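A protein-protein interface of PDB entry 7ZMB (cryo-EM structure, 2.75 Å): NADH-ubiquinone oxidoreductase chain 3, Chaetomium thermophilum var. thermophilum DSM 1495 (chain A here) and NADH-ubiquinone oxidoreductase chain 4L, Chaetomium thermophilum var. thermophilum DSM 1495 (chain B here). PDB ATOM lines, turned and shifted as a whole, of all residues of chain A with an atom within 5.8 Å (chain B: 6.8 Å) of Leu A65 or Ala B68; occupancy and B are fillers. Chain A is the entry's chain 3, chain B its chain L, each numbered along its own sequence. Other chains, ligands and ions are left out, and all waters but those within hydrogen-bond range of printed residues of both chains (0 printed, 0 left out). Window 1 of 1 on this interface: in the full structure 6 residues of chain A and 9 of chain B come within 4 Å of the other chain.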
ATOM      1  N   GLY A  60      19.980  25.654  13.353  1.00  0.00           N
ATOM      2  CA  GLY A  60      19.503  26.123  14.641  1.00  0.00           C
ATOM      3  C   GLY A  60      20.298  25.598  15.811  1.00  0.00           C
ATOM      4  O   GLY A  60      20.463  26.301  16.811  1.00  0.00           O
ATOM      5  N   LEU A  61      20.791  24.362  15.713  1.00  0.00           N
ATOM      6  CA  LEU A  61      21.628  23.804  16.766  1.00  0.00           C
ATOM      7  C   LEU A  61      22.976  24.508  16.830  1.00  0.00           C
ATOM      8  O   LEU A  61      23.441  24.877  17.913  1.00  0.00           O
ATOM      9  CB  LEU A  61      21.811  22.299  16.547  1.00  0.00           C
ATOM     10  CG  LEU A  61      20.604  21.389  16.781  1.00  0.00           C
ATOM     11  CD1 LEU A  61      20.790  20.026  16.148  1.00  0.00           C
ATOM     12  CD2 LEU A  61      20.335  21.238  18.256  1.00  0.00           C
ATOM     13  N   VAL A  62      23.626  24.706  15.680  1.00  0.00           N
ATOM     14  CA  VAL A  62      24.926  25.374  15.679  1.00  0.00           C
ATOM     15  C   VAL A  62      24.784  26.859  15.984  1.00  0.00           C
ATOM     16  O   VAL A  62      25.671  27.453  16.603  1.00  0.00           O
ATOM     17  CB  VAL A  62      25.681  25.128  14.358  1.00  0.00           C
ATOM     18  CG1 VAL A  62      25.689  23.670  14.022  1.00  0.00           C
ATOM     19  CG2 VAL A  62      25.063  25.908  13.222  1.00  0.00           C
ATOM     20  N   PHE A  63      23.681  27.485  15.561  1.00  0.00           N
ATOM     21  CA  PHE A  63      23.425  28.870  15.939  1.00  0.00           C
ATOM     22  C   PHE A  63      23.354  29.028  17.447  1.00  0.00           C
ATOM     23  O   PHE A  63      23.778  30.053  17.987  1.00  0.00           O
ATOM     24  CB  PHE A  63      22.125  29.360  15.307  1.00  0.00           C
ATOM     25  CG  PHE A  63      21.445  30.434  16.093  1.00  0.00           C
ATOM     26  CD1 PHE A  63      21.886  31.733  16.026  1.00  0.00           C
ATOM     27  CD2 PHE A  63      20.393  30.139  16.929  1.00  0.00           C
ATOM     28  CE1 PHE A  63      21.282  32.711  16.753  1.00  0.00           C
ATOM     29  CE2 PHE A  63      19.789  31.118  17.662  1.00  0.00           C
ATOM     30  CZ  PHE A  63      20.233  32.410  17.573  1.00  0.00           C
ATOM     31  N   LEU A  64      22.822  28.024  18.140  1.00  0.00           N
ATOM     32  CA  LEU A  64      22.695  28.069  19.590  1.00  0.00           C
ATOM     33  C   LEU A  64      24.053  28.230  20.257  1.00  0.00           C
ATOM     34  O   LEU A  64      24.205  29.035  21.180  1.00  0.00           O
ATOM     35  CB  LEU A  64      22.021  26.790  20.082  1.00  0.00           C
ATOM     36  CG  LEU A  64      20.508  26.676  20.227  1.00  0.00           C
ATOM     37  CD1 LEU A  64      20.144  25.220  20.294  1.00  0.00           C
ATOM     38  CD2 LEU A  64      19.995  27.385  21.442  1.00  0.00           C
ATOM     39  N   LEU A  65      25.033  27.441  19.813  1.00  0.00           N
ATOM     40  CA  LEU A  65      26.370  27.423  20.459  1.00  0.00           C
ATOM     41  C   LEU A  65      27.282  28.560  19.988  1.00  0.00           C
ATOM     42  O   LEU A  65      28.121  28.973  20.794  1.00  0.00           O
ATOM     43  CB  LEU A  65      27.000  26.063  20.165  1.00  0.00           C
ATOM     44  CG  LEU A  65      26.105  24.861  20.456  1.00  0.00           C
ATOM     45  CD1 LEU A  65      26.502  23.667  19.606  1.00  0.00           C
ATOM     46  CD2 LEU A  65      26.127  24.510  21.935  1.00  0.00           C
ATOM     47  N   LEU A  66      27.126  29.078  18.769  1.00  0.00           N
ATOM     48  CA  LEU A  66      28.092  30.115  18.320  1.00  0.00           C
ATOM     49  C   LEU A  66      27.659  31.433  18.950  1.00  0.00           C
ATOM     50  O   LEU A  66      28.509  32.320  19.080  1.00  0.00           O
ATOM     51  CB  LEU A  66      28.160  30.165  16.792  1.00  0.00           C
ATOM     52  CG  LEU A  66      29.237  29.283  16.163  1.00  0.00           C
ATOM     53  CD1 LEU A  66      29.072  29.202  14.662  1.00  0.00           C
ATOM     54  CD2 LEU A  66      30.621  29.803  16.497  1.00  0.00           C
ATOM     55  N   ASP A  67      26.394  31.538  19.347  1.00  0.00           N
ATOM     56  CA  ASP A  67      25.921  32.718  20.112  1.00  0.00           C
ATOM     57  C   ASP A  67      26.627  32.733  21.472  1.00  0.00           C
ATOM     58  O   ASP A  67      27.066  33.805  21.885  1.00  0.00           O
ATOM     59  CB  ASP A  67      24.410  32.620  20.308  1.00  0.00           C
ATOM     60  CG  ASP A  67      23.696  33.927  20.600  1.00  0.00           C
ATOM     61  OD1 ASP A  67      24.381  34.939  20.827  1.00  0.00           O
ATOM     62  OD2 ASP A  67      22.449  33.919  20.591  1.00  0.00           O
ATOM     63  N   LEU A  68      26.703  31.586  22.140  1.00  0.00           N
ATOM     64  CA  LEU A  68      27.377  31.488  23.458  1.00  0.00           C
ATOM     65  C   LEU A  68      28.839  31.883  23.268  1.00  0.00           C
ATOM     66  O   LEU A  68      29.373  32.601  24.132  1.00  0.00           O
ATOM     67  CB  LEU A  68      27.258  30.046  23.945  1.00  0.00           C
ATOM     68  CG  LEU A  68      25.834  29.531  24.143  1.00  0.00           C
ATOM     69  CD1 LEU A  68      25.816  28.022  24.307  1.00  0.00           C
ATOM     70  CD2 LEU A  68      25.170  30.203  25.331  1.00  0.00           C
ATOM     71  N   GLU A  69      29.436  31.469  22.152  1.00  0.00           N
ATOM     72  CA  GLU A  69      30.856  31.772  21.855  1.00  0.00           C
ATOM     73  C   GLU A  69      31.124  33.269  21.643  1.00  0.00           C
ATOM     74  O   GLU A  69      32.168  33.735  22.131  1.00  0.00           O
ATOM     75  CB  GLU A  69      31.323  30.833  20.747  1.00  0.00           C
ATOM     76  CG  GLU A  69      31.522  29.419  21.265  1.00  0.00           C
ATOM     77  CD  GLU A  69      31.277  28.268  20.305  1.00  0.00           C
ATOM     78  OE1 GLU A  69      30.686  28.500  19.245  1.00  0.00           O
ATOM     79  OE2 GLU A  69      31.686  27.137  20.623  1.00  0.00           O
ATOM     80  N   ILE A  70      30.242  34.002  20.953  1.00  0.00           N
ATOM     81  CA  ILE A  70      30.547  35.435  20.633  1.00  0.00           C
ATOM     82  C   ILE A  70      30.187  36.260  21.866  1.00  0.00           C
ATOM     83  O   ILE A  70      30.837  37.290  22.094  1.00  0.00           O
ATOM     84  CB  ILE A  70      29.823  35.892  19.347  1.00  0.00           C
ATOM     85  CG1 ILE A  70      30.173  34.995  18.157  1.00  0.00           C
ATOM     86  CG2 ILE A  70      30.097  37.355  19.035  1.00  0.00           C
ATOM     87  CD1 ILE A  70      29.276  35.188  16.961  1.00  0.00           C
ATOM     88  N   LEU B  26      12.974  18.615  28.721  1.00  0.00           N
ATOM     89  CA  LEU B  26      14.199  19.362  28.485  1.00  0.00           C
ATOM     90  C   LEU B  26      14.045  20.840  28.834  1.00  0.00           C
ATOM     91  O   LEU B  26      15.030  21.497  29.182  1.00  0.00           O
ATOM     92  CB  LEU B  26      14.599  19.149  27.027  1.00  0.00           C
ATOM     93  CG  LEU B  26      15.602  19.965  26.232  1.00  0.00           C
ATOM     94  CD1 LEU B  26      17.019  19.710  26.688  1.00  0.00           C
ATOM     95  CD2 LEU B  26      15.433  19.590  24.781  1.00  0.00           C
ATOM     96  N   VAL B  61      26.413  28.990  29.502  1.00  0.00           N
ATOM     97  CA  VAL B  61      27.083  28.391  28.300  1.00  0.00           C
ATOM     98  C   VAL B  61      26.920  26.872  28.305  1.00  0.00           C
ATOM     99  O   VAL B  61      26.674  26.318  27.225  1.00  0.00           O
ATOM    100  CB  VAL B  61      28.561  28.815  28.103  1.00  0.00           C
ATOM    101  CG1 VAL B  61      29.522  28.100  29.037  1.00  0.00           C
ATOM    102  CG2 VAL B  61      29.022  28.662  26.672  1.00  0.00           C
ATOM    103  N   ALA B  63      24.468  25.326  29.908  1.00  0.00           N
ATOM    104  CA  ALA B  63      23.045  25.030  29.835  1.00  0.00           C
ATOM    105  C   ALA B  63      22.549  25.080  28.400  1.00  0.00           C
ATOM    106  O   ALA B  63      21.540  24.451  28.071  1.00  0.00           O
ATOM    107  CB  ALA B  63      22.252  26.003  30.712  1.00  0.00           C
ATOM    108  N   GLY B  64      23.234  25.830  27.544  1.00  0.00           N
ATOM    109  CA  GLY B  64      22.922  25.863  26.134  1.00  0.00           C
ATOM    110  C   GLY B  64      23.556  24.701  25.412  1.00  0.00           C
ATOM    111  O   GLY B  64      22.977  24.159  24.470  1.00  0.00           O
ATOM    112  N   ALA B  65      24.751  24.307  25.852  1.00  0.00           N
ATOM    113  CA  ALA B  65      25.373  23.104  25.318  1.00  0.00           C
ATOM    114  C   ALA B  65      24.529  21.873  25.621  1.00  0.00           C
ATOM    115  O   ALA B  65      24.366  20.995  24.766  1.00  0.00           O
ATOM    116  CB  ALA B  65      26.780  22.943  25.884  1.00  0.00           C
ATOM    117  N   GLU B  66      23.981  21.796  26.834  1.00  0.00           N
ATOM    118  CA  GLU B  66      23.111  20.680  27.181  1.00  0.00           C
ATOM    119  C   GLU B  66      21.855  20.668  26.319  1.00  0.00           C
ATOM    120  O   GLU B  66      21.438  19.609  25.840  1.00  0.00           O
ATOM    121  CB  GLU B  66      22.742  20.740  28.663  1.00  0.00           C
ATOM    122  CG  GLU B  66      21.699  19.719  29.075  1.00  0.00           C
ATOM    123  CD  GLU B  66      21.322  19.811  30.534  1.00  0.00           C
ATOM    124  OE1 GLU B  66      21.375  20.924  31.093  1.00  0.00           O
ATOM    125  OE2 GLU B  66      20.976  18.768  31.123  1.00  0.00           O
ATOM    126  N   SER B  67      21.243  21.832  26.101  1.00  0.00           N
ATOM    127  CA  SER B  67      19.998  21.874  25.341  1.00  0.00           C
ATOM    128  C   SER B  67      20.211  21.628  23.853  1.00  0.00           C
ATOM    129  O   SER B  67      19.282  21.184  23.175  1.00  0.00           O
ATOM    130  CB  SER B  67      19.281  23.206  25.563  1.00  0.00           C
ATOM    131  OG  SER B  67      20.083  24.304  25.172  1.00  0.00           O
ATOM    132  N   ALA B  68      21.405  21.902  23.332  1.00  0.00           N
ATOM    133  CA  ALA B  68      21.708  21.519  21.959  1.00  0.00           C
ATOM    134  C   ALA B  68      21.950  20.018  21.845  1.00  0.00           C
ATOM    135  O   ALA B  68      21.463  19.375  20.910  1.00  0.00           O
ATOM    136  CB  ALA B  68      22.914  22.301  21.448  1.00  0.00           C
ATOM    137  N   ILE B  69      22.688  19.441  22.792  1.00  0.00           N
ATOM    138  CA  ILE B  69      22.898  17.998  22.787  1.00  0.00           C
ATOM    139  C   ILE B  69      21.580  17.276  23.015  1.00  0.00           C
ATOM    140  O   ILE B  69      21.329  16.212  22.438  1.00  0.00           O
ATOM    141  CB  ILE B  69      23.964  17.606  23.830  1.00  0.00           C
ATOM    142  CG1 ILE B  69      25.337  18.094  23.381  1.00  0.00           C
ATOM    143  CG2 ILE B  69      24.015  16.099  24.021  1.00  0.00           C
ATOM    144  CD1 ILE B  69      25.649  17.769  21.943  1.00  0.00           C
ATOM    145  N   GLY B  70      20.710  17.846  23.848  1.00  0.00           N
ATOM    146  CA  GLY B  70      19.401  17.252  24.045  1.00  0.00           C
ATOM    147  C   GLY B  70      18.550  17.278  22.791  1.00  0.00           C
ATOM    148  O   GLY B  70      18.002  16.256  22.381  1.00  0.00           O
ATOM    149  N   LEU B  71      18.435  18.447  22.158  1.00  0.00           N
ATOM    150  CA  LEU B  71      17.618  18.540  20.955  1.00  0.00           C
ATOM    151  C   LEU B  71      18.175  17.675  19.836  1.00  0.00           C
ATOM    152  O   LEU B  71      17.408  17.131  19.034  1.00  0.00           O
ATOM    153  CB  LEU B  71      17.490  19.996  20.501  1.00  0.00           C
ATOM    154  CG  LEU B  71      16.559  20.872  21.341  1.00  0.00           C
ATOM    155  CD1 LEU B  71      16.673  22.310  20.939  1.00  0.00           C
ATOM    156  CD2 LEU B  71      15.123  20.403  21.221  1.00  0.00           C
ATOM    157  N   GLY B  72      19.498  17.534  19.767  1.00  0.00           N
ATOM    158  CA  GLY B  72      20.085  16.627  18.795  1.00  0.00           C
ATOM    159  C   GLY B  72      19.745  15.173  19.064  1.00  0.00           C
ATOM    160  O   GLY B  72      19.453  14.416  18.136  1.00  0.00           O
ATOM    161  N   ILE B  73      19.789  14.760  20.329  1.00  0.00           N
ATOM    162  CA  ILE B  73      19.443  13.386  20.672  1.00  0.00           C
ATOM    163  C   ILE B  73      17.954  13.154  20.489  1.00  0.00           C
ATOM    164  O   ILE B  73      17.523  12.082  20.048  1.00  0.00           O
ATOM    165  CB  ILE B  73      19.908  13.061  22.102  1.00  0.00           C
ATOM    166  CG1 ILE B  73      21.419  12.831  22.118  1.00  0.00           C
ATOM    167  CG2 ILE B  73      19.197  11.830  22.632  1.00  0.00           C
ATOM    168  CD1 ILE B  73      22.035  12.826  23.484  1.00  0.00           C
ATOM    169  N   LEU B  74      17.144  14.160  20.824  1.00  0.00           N
ATOM    170  CA  LEU B  74      15.700  14.060  20.661  1.00  0.00           C
ATOM    171  C   LEU B  74      15.322  13.846  19.201  1.00  0.00           C
ATOM    172  O   LEU B  74      14.456  13.023  18.888  1.00  0.00           O
ATOM    173  CB  LEU B  74      15.053  15.322  21.216  1.00  0.00           C
ATOM    174  CG  LEU B  74      13.575  15.361  21.567  1.00  0.00           C
ATOM    175  CD1 LEU B  74      13.131  14.065  22.238  1.00  0.00           C
ATOM    176  CD2 LEU B  74      13.349  16.550  22.467  1.00  0.00           C
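Among the printed residues, pairs that only touch across the chains: Leu A61 with Ala B68 (3.4 Å), Leu A68 with Val B61 (3.5 Å), Leu A65 with Ala B65 (3.7 Å), Leu A61 with Leu B71 (3.8 Å) and Leu A65 with Ala B68 (3.9 Å).
Leu A65 touches two residues of chain B.
Of the printed residues of chain A, Ala B68 touches Leu A61 (3.4 Å) and Leu A65 (3.9 Å).
Of the printed residues of chain A, Ala B65 touches Leu A65.
Printed residues of chain A within 4 Å of Leu B71: Leu A61 (3.8 Å).
Of the printed residues of chain B, Leu A61 touches Ala B68 and Leu B71.
Printed residues of chain B within 4 Å of Leu A68: Val B61 (3.5 Å).
Gly B70 touches none of the printed residues of chain A.
Val A62 touches none of the printed residues of chain B.
The nearest residue of chain B that does not touch Leu A65 is Gly B64 (4.1 Å).
The nearest printed residue of chain A that does not touch Ala B65 is Leu A68 (4.2 Å).
Of the 14 printed residues of chain B, 4 touch a printed residue of chain A.
Hydrophobic or aromatic side chains of chain A that line the printed part of chain B: Leu A61, Leu A65 and Leu A68.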
